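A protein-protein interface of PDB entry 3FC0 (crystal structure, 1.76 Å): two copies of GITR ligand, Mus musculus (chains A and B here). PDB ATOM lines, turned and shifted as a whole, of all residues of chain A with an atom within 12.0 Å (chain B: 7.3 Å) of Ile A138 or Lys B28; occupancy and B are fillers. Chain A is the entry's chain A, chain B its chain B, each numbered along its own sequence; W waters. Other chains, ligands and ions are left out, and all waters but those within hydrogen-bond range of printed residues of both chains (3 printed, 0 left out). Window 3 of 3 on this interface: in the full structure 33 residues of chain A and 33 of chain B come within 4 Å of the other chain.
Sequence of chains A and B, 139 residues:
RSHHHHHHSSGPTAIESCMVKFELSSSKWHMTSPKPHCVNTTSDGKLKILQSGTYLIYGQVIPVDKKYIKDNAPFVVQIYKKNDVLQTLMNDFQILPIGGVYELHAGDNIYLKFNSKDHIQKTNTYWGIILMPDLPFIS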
ATOM      1  N   PRO A 133      -9.922 -18.452 -31.412  1.00  0.00           N
ATOM      2  CA  PRO A 133     -10.074 -19.412 -30.303  1.00  0.00           C
ATOM      3  C   PRO A 133     -10.782 -18.745 -29.113  1.00  0.00           C
ATOM      4  O   PRO A 133     -10.818 -17.511 -29.033  1.00  0.00           O
ATOM      5  CB  PRO A 133      -8.637 -19.780 -29.962  1.00  0.00           C
ATOM      6  CG  PRO A 133      -7.795 -18.574 -30.369  1.00  0.00           C
ATOM      7  CD  PRO A 133      -8.524 -18.049 -31.637  1.00  0.00           C
ATOM      8  N   ASP A 134     -11.381 -19.532 -28.214  1.00  0.00           N
ATOM      9  CA  ASP A 134     -11.931 -18.963 -26.994  1.00  0.00           C
ATOM     10  C   ASP A 134     -10.765 -18.380 -26.232  1.00  0.00           C
ATOM     11  O   ASP A 134      -9.629 -18.859 -26.372  1.00  0.00           O
ATOM     12  CB  ASP A 134     -12.645 -20.026 -26.131  1.00  0.00           C
ATOM     13  CG  ASP A 134     -13.887 -20.595 -26.796  1.00  0.00           C
ATOM     14  OD1 ASP A 134     -14.702 -19.824 -27.358  1.00  0.00           O
ATOM     15  OD2 ASP A 134     -14.059 -21.842 -26.755  1.00  0.00           O
ATOM     16  N   LEU A 135     -11.025 -17.333 -25.440  1.00  0.00           N
ATOM     17  CA  LEU A 135      -9.981 -16.689 -24.646  1.00  0.00           C
ATOM     18  C   LEU A 135     -10.476 -16.699 -23.201  1.00  0.00           C
ATOM     19  O   LEU A 135     -10.752 -15.637 -22.621  1.00  0.00           O
ATOM     20  CB  LEU A 135      -9.719 -15.230 -25.076  1.00  0.00           C
ATOM     21  CG  LEU A 135      -9.495 -14.962 -26.579  1.00  0.00           C
ATOM     22  CD1 LEU A 135      -9.275 -13.444 -26.861  1.00  0.00           C
ATOM     23  CD2 LEU A 135      -8.292 -15.730 -26.974  1.00  0.00           C
ATOM     24  N   PRO A 136     -10.597 -17.906 -22.618  1.00  0.00           N
ATOM     25  CA  PRO A 136     -11.179 -18.028 -21.282  1.00  0.00           C
ATOM     26  C   PRO A 136     -10.288 -17.556 -20.114  1.00  0.00           C
ATOM     27  O   PRO A 136     -10.819 -17.205 -19.053  1.00  0.00           O
ATOM     28  CB  PRO A 136     -11.526 -19.531 -21.187  1.00  0.00           C
ATOM     29  CG  PRO A 136     -10.552 -20.210 -22.104  1.00  0.00           C
ATOM     30  CD  PRO A 136     -10.141 -19.196 -23.168  1.00  0.00           C
ATOM     31  N   PHE A 137      -8.972 -17.540 -20.265  1.00  0.00           N
ATOM     32  CA  PHE A 137      -8.107 -17.190 -19.150  1.00  0.00           C
ATOM     33  C   PHE A 137      -7.802 -15.710 -19.079  1.00  0.00           C
ATOM     34  O   PHE A 137      -7.553 -15.073 -20.112  1.00  0.00           O
ATOM     35  CB  PHE A 137      -6.843 -18.020 -19.199  1.00  0.00           C
ATOM     36  CG  PHE A 137      -7.144 -19.480 -19.181  1.00  0.00           C
ATOM     37  CD1 PHE A 137      -7.485 -20.103 -17.980  1.00  0.00           C
ATOM     38  CD2 PHE A 137      -7.185 -20.208 -20.358  1.00  0.00           C
ATOM     39  CE1 PHE A 137      -7.790 -21.444 -17.949  1.00  0.00           C
ATOM     40  CE2 PHE A 137      -7.491 -21.553 -20.340  1.00  0.00           C
ATOM     41  CZ  PHE A 137      -7.810 -22.174 -19.135  1.00  0.00           C
ATOM     42  N   ILE A 138      -7.872 -15.167 -17.863  1.00  0.00           N
ATOM     43  CA  ILE A 138      -7.817 -13.705 -17.661  1.00  0.00           C
ATOM     44  C   ILE A 138      -6.699 -13.431 -16.689  1.00  0.00           C
ATOM     45  O   ILE A 138      -6.588 -14.112 -15.657  1.00  0.00           O
ATOM     46  CB  ILE A 138      -9.154 -13.151 -17.140  1.00  0.00           C
ATOM     47  CG1 ILE A 138     -10.265 -13.363 -18.199  1.00  0.00           C
ATOM     48  CG2 ILE A 138      -9.009 -11.645 -16.805  1.00  0.00           C
ATOM     49  CD1 ILE A 138     -11.659 -13.108 -17.690  1.00  0.00           C
ATOM     50  N   SER A 139      -5.844 -12.457 -16.996  1.00  0.00           N
ATOM     51  CA  SER A 139      -4.739 -12.156 -16.124  1.00  0.00           C
ATOM     52  C   SER A 139      -4.340 -10.678 -16.168  1.00  0.00           C
ATOM     53  O   SER A 139      -4.388 -10.024 -17.223  1.00  0.00           O
ATOM     54  CB  SER A 139      -3.545 -13.000 -16.524  1.00  0.00           C
ATOM     55  OG  SER A 139      -2.519 -12.868 -15.562  1.00  0.00           O
ATOM     56  OXT SER A 139      -3.948 -10.122 -15.145  1.00  0.00           O
ATOM     57  N   LYS B  21      -5.626 -10.764 -25.776  1.00  0.00           N
ATOM     58  CA  LYS B  21      -6.352  -9.514 -26.005  1.00  0.00           C
ATOM     59  C   LYS B  21      -6.380  -8.705 -24.729  1.00  0.00           C
ATOM     60  O   LYS B  21      -6.946  -9.159 -23.704  1.00  0.00           O
ATOM     61  CB  LYS B  21      -7.772  -9.841 -26.412  1.00  0.00           C
ATOM     62  CG  LYS B  21      -8.627  -8.627 -26.713  1.00  0.00           C
ATOM     63  CD  LYS B  21     -10.038  -9.079 -26.916  1.00  0.00           C
ATOM     64  CE  LYS B  21     -10.912  -8.010 -27.545  1.00  0.00           C
ATOM     65  NZ  LYS B  21     -12.347  -8.237 -27.097  1.00  0.00           N
ATOM     66  N   PHE B  22      -5.834  -7.495 -24.793  1.00  0.00           N
ATOM     67  CA  PHE B  22      -5.809  -6.593 -23.643  1.00  0.00           C
ATOM     68  C   PHE B  22      -7.051  -5.699 -23.677  1.00  0.00           C
ATOM     69  O   PHE B  22      -7.338  -5.084 -24.684  1.00  0.00           O
ATOM     70  CB  PHE B  22      -4.539  -5.752 -23.695  1.00  0.00           C
ATOM     71  CG  PHE B  22      -4.331  -4.882 -22.473  1.00  0.00           C
ATOM     72  CD1 PHE B  22      -3.936  -5.434 -21.267  1.00  0.00           C
ATOM     73  CD2 PHE B  22      -4.526  -3.501 -22.548  1.00  0.00           C
ATOM     74  CE1 PHE B  22      -3.726  -4.632 -20.134  1.00  0.00           C
ATOM     75  CE2 PHE B  22      -4.314  -2.684 -21.405  1.00  0.00           C
ATOM     76  CZ  PHE B  22      -3.908  -3.264 -20.210  1.00  0.00           C
ATOM     77  N   GLU B  23      -7.810  -5.657 -22.588  1.00  0.00           N
ATOM     78  CA  GLU B  23      -8.978  -4.777 -22.484  1.00  0.00           C
ATOM     79  C   GLU B  23      -8.579  -3.565 -21.636  1.00  0.00           C
ATOM     80  O   GLU B  23      -8.214  -3.712 -20.455  1.00  0.00           O
ATOM     81  CB  GLU B  23     -10.140  -5.481 -21.806  1.00  0.00           C
ATOM     82  CG  GLU B  23     -10.646  -6.667 -22.570  1.00  0.00           C
ATOM     83  CD  GLU B  23     -11.456  -6.268 -23.782  1.00  0.00           C
ATOM     84  OE1 GLU B  23     -11.888  -5.092 -23.876  1.00  0.00           O
ATOM     85  OE2 GLU B  23     -11.677  -7.145 -24.645  1.00  0.00           O
ATOM     86  N   LEU B  24      -8.589  -2.384 -22.233  1.00  0.00           N
ATOM     87  CA  LEU B  24      -8.152  -1.192 -21.514  1.00  0.00           C
ATOM     88  C   LEU B  24      -9.083  -0.862 -20.344  1.00  0.00           C
ATOM     89  O   LEU B  24      -8.653  -0.317 -19.344  1.00  0.00           O
ATOM     90  CB  LEU B  24      -8.062   0.005 -22.476  1.00  0.00           C
ATOM     91  CG  LEU B  24      -7.344   1.227 -21.922  1.00  0.00           C
ATOM     92  CD1 LEU B  24      -5.952   0.846 -21.508  1.00  0.00           C
ATOM     93  CD2 LEU B  24      -7.274   2.330 -23.004  1.00  0.00           C
ATOM     94  N   SER B  25     -10.343  -1.209 -20.441  1.00  0.00           N
ATOM     95  CA  SER B  25     -11.232  -0.857 -19.352  1.00  0.00           C
ATOM     96  C   SER B  25     -10.833  -1.536 -18.036  1.00  0.00           C
ATOM     97  O   SER B  25     -10.923  -0.923 -16.975  1.00  0.00           O
ATOM     98  CB  SER B  25     -12.669  -1.143 -19.714  1.00  0.00           C
ATOM     99  OG  SER B  25     -12.842  -2.509 -20.019  1.00  0.00           O
ATOM    100  N   SER B  26     -10.335  -2.766 -18.095  1.00  0.00           N
ATOM    101  CA  SER B  26     -10.070  -3.497 -16.867  1.00  0.00           C
ATOM    102  C   SER B  26      -8.580  -3.678 -16.680  1.00  0.00           C
ATOM    103  O   SER B  26      -8.118  -4.077 -15.619  1.00  0.00           O
ATOM    104  CB  SER B  26     -10.791  -4.840 -16.906  1.00  0.00           C
ATOM    105  OG  SER B  26     -10.306  -5.607 -17.988  1.00  0.00           O
ATOM    106  N   SER B  27      -7.801  -3.365 -17.715  1.00  0.00           N
ATOM    107  CA  SER B  27      -6.382  -3.629 -17.679  1.00  0.00           C
ATOM    108  C   SER B  27      -6.004  -5.111 -17.507  1.00  0.00           C
ATOM    109  O   SER B  27      -4.976  -5.433 -16.911  1.00  0.00           O
ATOM    110  CB  SER B  27      -5.699  -2.779 -16.607  1.00  0.00           C
ATOM    111  OG  SER B  27      -5.484  -1.458 -17.098  1.00  0.00           O
ATOM    112  N   LYS B  28      -6.812  -5.987 -18.080  1.00  0.00           N
ATOM    113  CA  LYS B  28      -6.573  -7.423 -18.027  1.00  0.00           C
ATOM    114  C   LYS B  28      -6.444  -7.977 -19.433  1.00  0.00           C
ATOM    115  O   LYS B  28      -7.109  -7.489 -20.357  1.00  0.00           O
ATOM    116  CB  LYS B  28      -7.773  -8.100 -17.411  1.00  0.00           C
ATOM    117  CG  LYS B  28      -8.178  -7.549 -16.047  1.00  0.00           C
ATOM    118  CD  LYS B  28      -7.191  -7.983 -15.049  1.00  0.00           C
ATOM    119  CE  LYS B  28      -7.677  -7.678 -13.593  1.00  0.00           C
ATOM    120  NZ  LYS B  28      -6.486  -7.775 -12.730  1.00  0.00           N
ATOM    121  N   TRP B  29      -5.627  -9.017 -19.566  1.00  0.00           N
ATOM    122  CA  TRP B  29      -5.475  -9.748 -20.803  1.00  0.00           C
ATOM    123  C   TRP B  29      -6.367 -10.985 -20.766  1.00  0.00           C
ATOM    124  O   TRP B  29      -6.414 -11.689 -19.739  1.00  0.00           O
ATOM    125  CB  TRP B  29      -4.047 -10.204 -20.957  1.00  0.00           C
ATOM    126  CG  TRP B  29      -3.045  -9.129 -21.191  1.00  0.00           C
ATOM    127  CD1 TRP B  29      -2.324  -8.424 -20.251  1.00  0.00           C
ATOM    128  CD2 TRP B  29      -2.610  -8.663 -22.456  1.00  0.00           C
ATOM    129  NE1 TRP B  29      -1.432  -7.571 -20.867  1.00  0.00           N
ATOM    130  CE2 TRP B  29      -1.611  -7.682 -22.223  1.00  0.00           C
ATOM    131  CE3 TRP B  29      -2.977  -8.967 -23.772  1.00  0.00           C
ATOM    132  CZ2 TRP B  29      -0.988  -7.018 -23.251  1.00  0.00           C
ATOM    133  CZ3 TRP B  29      -2.358  -8.294 -24.780  1.00  0.00           C
ATOM    134  CH2 TRP B  29      -1.370  -7.346 -24.520  1.00  0.00           C
ATOM    135  N   HIS B  30      -7.046 -11.247 -21.881  1.00  0.00           N
ATOM    136  CA  HIS B  30      -7.850 -12.446 -22.088  1.00  0.00           C
ATOM    137  C   HIS B  30      -7.040 -13.328 -22.999  1.00  0.00           C
ATOM    138  O   HIS B  30      -6.442 -12.845 -23.981  1.00  0.00           O
ATOM    139  CB  HIS B  30      -9.211 -12.044 -22.678  1.00  0.00           C
ATOM    140  CG  HIS B  30     -10.041 -11.209 -21.756  1.00  0.00           C
ATOM    141  ND1 HIS B  30     -11.298 -11.593 -21.351  1.00  0.00           N
ATOM    142  CD2 HIS B  30      -9.789 -10.035 -21.127  1.00  0.00           C
ATOM    143  CE1 HIS B  30     -11.800 -10.683 -20.531  1.00  0.00           C
ATOM    144  NE2 HIS B  30     -10.895  -9.736 -20.363  1.00  0.00           N
ATOM    145  N   MET B  31      -6.933 -14.630 -22.669  1.00  0.00           N
ATOM    146  CA  MET B  31      -5.863 -15.420 -23.267  1.00  0.00           C
ATOM    147  C   MET B  31      -6.302 -16.853 -23.565  1.00  0.00           C
ATOM    148  O   MET B  31      -7.276 -17.334 -23.003  1.00  0.00           O
ATOM    149  CB  MET B  31      -4.627 -15.469 -22.358  1.00  0.00           C
ATOM    150  CG  MET B  31      -4.232 -14.106 -21.704  1.00  0.00           C
ATOM    151  SD  MET B  31      -2.865 -14.435 -20.534  1.00  0.00           S
ATOM    152  CE  MET B  31      -3.768 -15.450 -19.370  1.00  0.00           C
ATOM    153  N   SER B  33      -4.649 -19.557 -23.033  1.00  0.00           N
ATOM    154  CA  SER B  33      -4.247 -20.411 -21.906  1.00  0.00           C
ATOM    155  C   SER B  33      -3.621 -19.554 -20.780  1.00  0.00           C
ATOM    156  O   SER B  33      -3.397 -18.376 -20.950  1.00  0.00           O
ATOM    157  CB  SER B  33      -3.254 -21.433 -22.429  1.00  0.00           C
ATOM    158  OG  SER B  33      -2.003 -20.812 -22.553  1.00  0.00           O
ATOM    159  N   PRO B  34      -3.339 -20.152 -19.599  1.00  0.00           N
ATOM    160  CA  PRO B  34      -2.759 -19.388 -18.489  1.00  0.00           C
ATOM    161  C   PRO B  34      -1.397 -18.793 -18.791  1.00  0.00           C
ATOM    162  O   PRO B  34      -1.060 -17.708 -18.298  1.00  0.00           O
ATOM    163  CB  PRO B  34      -2.626 -20.459 -17.374  1.00  0.00           C
ATOM    164  CG  PRO B  34      -3.800 -21.364 -17.629  1.00  0.00           C
ATOM    165  CD  PRO B  34      -3.866 -21.462 -19.165  1.00  0.00           C
ATOM    166  N   THR B  42       2.137  -7.995 -19.943  1.00  0.00           N
ATOM    167  CA  THR B  42       2.338  -7.140 -18.768  1.00  0.00           C
ATOM    168  C   THR B  42       1.051  -6.383 -18.401  1.00  0.00           C
ATOM    169  O   THR B  42       0.228  -6.082 -19.263  1.00  0.00           O
ATOM    170  CB  THR B  42       3.478  -6.138 -19.029  1.00  0.00           C
ATOM    171  OG1 THR B  42       2.962  -5.005 -19.738  1.00  0.00           O
ATOM    172  CG2 THR B  42       4.567  -6.777 -19.860  1.00  0.00           C
ATOM    173  N   SER B  43       0.867  -6.062 -17.121  1.00  0.00           N
ATOM    174  CA  SER B  43      -0.386  -5.438 -16.677  1.00  0.00           C
ATOM    175  C   SER B  43      -0.525  -4.004 -17.184  1.00  0.00           C
ATOM    176  O   SER B  43      -1.595  -3.404 -17.084  1.00  0.00           O
ATOM    177  CB  SER B  43      -0.504  -5.466 -15.141  1.00  0.00           C
ATOM    178  OG  SER B  43       0.438  -4.576 -14.582  1.00  0.00           O
ATOM    179  N   TRP B 127      -6.411  -4.261 -27.592  1.00  0.00           N
ATOM    180  CA  TRP B 127      -5.447  -4.619 -28.613  1.00  0.00           C
ATOM    181  C   TRP B 127      -4.813  -5.945 -28.222  1.00  0.00           C
ATOM    182  O   TRP B 127      -4.958  -6.426 -27.074  1.00  0.00           O
ATOM    183  CB  TRP B 127      -4.380  -3.537 -28.750  1.00  0.00           C
ATOM    184  CG  TRP B 127      -3.646  -3.237 -27.489  1.00  0.00           C
ATOM    185  CD1 TRP B 127      -2.575  -3.897 -27.001  1.00  0.00           C
ATOM    186  CD2 TRP B 127      -3.886  -2.130 -26.595  1.00  0.00           C
ATOM    187  NE1 TRP B 127      -2.143  -3.309 -25.844  1.00  0.00           N
ATOM    188  CE2 TRP B 127      -2.918  -2.208 -25.580  1.00  0.00           C
ATOM    189  CE3 TRP B 127      -4.824  -1.076 -26.568  1.00  0.00           C
ATOM    190  CZ2 TRP B 127      -2.845  -1.272 -24.534  1.00  0.00           C
ATOM    191  CZ3 TRP B 127      -4.767  -0.151 -25.520  1.00  0.00           C
ATOM    192  CH2 TRP B 127      -3.782  -0.266 -24.512  1.00  0.00           C
HETATM  193  O   HOH W   1      -4.833 -10.220 -12.672  1.00  0.00           O
HETATM  194  O   HOH W   2     -12.379 -13.770 -22.160  1.00  0.00           O
HETATM  195  O   HOH W   3      -2.604  -7.716 -16.319  1.00  0.00           O
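Among the printed residues, 15 pairs touch across the chains.
Among the printed residues, no Asp or Glu carboxylate lies within 4 Å of a Lys or Arg side-chain nitrogen of the other chain.
Water W2 bridges the backbone carbonyl oxygen of Leu A135 and a ring nitrogen (ND1) of His B30.
Water W1 lies within hydrogen-bond range of the chain-end carboxylate (OXT) of Ser A139 (2.6 Å) and the side-chain amino group (NZ) of Lys B28 (3.0 Å).
Water W3 lies within hydrogen-bond range of OXT of Ser A139 (3.0 Å) and O of Ser B27 (3.3 Å).
Among the printed residues, merely in contact across the chains: Ile A138 with Trp B29 (3.2 Å), Leu A135 with Met B31 (3.2 Å), Phe A137 with His B30 (3.3 Å), Phe A137 with Ser B33 (3.3 Å), Ser A139 with Lys B28 (3.5 Å), Phe A137 with Trp B29 (3.6 Å), Ile A138 with His B30 (3.7 Å), Phe A137 with Pro B34 (3.7 Å), Ser A139 with Met B31 (3.8 Å), Ile A138 with Lys B28 (3.8 Å), Leu A135 with His B30 (3.9 Å) and Leu A135 with Lys B21 (3.9 Å).
O of Phe A137 lies within hydrogen-bond range of N of Met B31 (2.7 Å).
The backbone NH (N) of Trp B29 is in hydrogen-bond range of the chain-end carboxylate (O) of Ser A139 (2.8 Å).
The backbone carbonyl oxygen of Met B31 lies close to the backbone nitrogen of Pro A136 (3.4 Å).
Asp A134 touches none of the printed residues of chain B.
Of the printed residues of chain B, Leu A135 touches Lys B21, His B30 and Met B31.
Of the printed residues of chain B, Pro A136 touches Met B31.
Printed residues of chain B within 4 Å of Phe A137: Trp B29, His B30, Met B31, Ser B33 and Pro B34.
Printed residues of chain A within 4 Å of Lys B21: Leu A135 (3.9 Å).
No residue of chain A comes within 4 Å of Glu B23.
No residue of chain A comes within 4 Å of Ser B26.
No residue of chain A comes within 4 Å of Ser B27.
Of chain A, only Ile A138 and Ser A139 come within 4 Å of Lys B28.
Of chain A, only Phe A137 (3.6 Å), Ile A138 (3.2 Å) and Ser A139 (2.8 Å) come within 4 Å of Trp B29.
Of the printed residues of chain A, Ser B33 touches Phe A137.
Printed residues of chain A within 4 Å of Pro B34: Phe A137 (3.7 Å).
Trp B127 touches none of the printed residues of chain A.
The nearest residue of chain A that does not touch Lys B28 is Phe A137 (7.2 Å).
The nearest printed residue of chain A that does not touch Lys B21 is Phe A137 (6.9 Å).
No position is printed for both chains.
Of the 15 pairs that touch across the chains among the printed residues, none has its exchanged pair printed and touching as well.
OE2 of Glu B23 lies within salt-bridge range of NZ of Lys B21 (2.8 Å).
The backbone carbonyl oxygen (O) of Lys B21 sits at hydrogen-bond distance from the backbone NH (N) of His B30 (2.8 Å).
N of Glu B23 lies within hydrogen-bond range of O of Lys B28 (3.0 Å).
The indole nitrogen of Trp B29 sits at hydrogen-bond distance from the backbone carbonyl oxygen of Thr B42 (2.7 Å).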
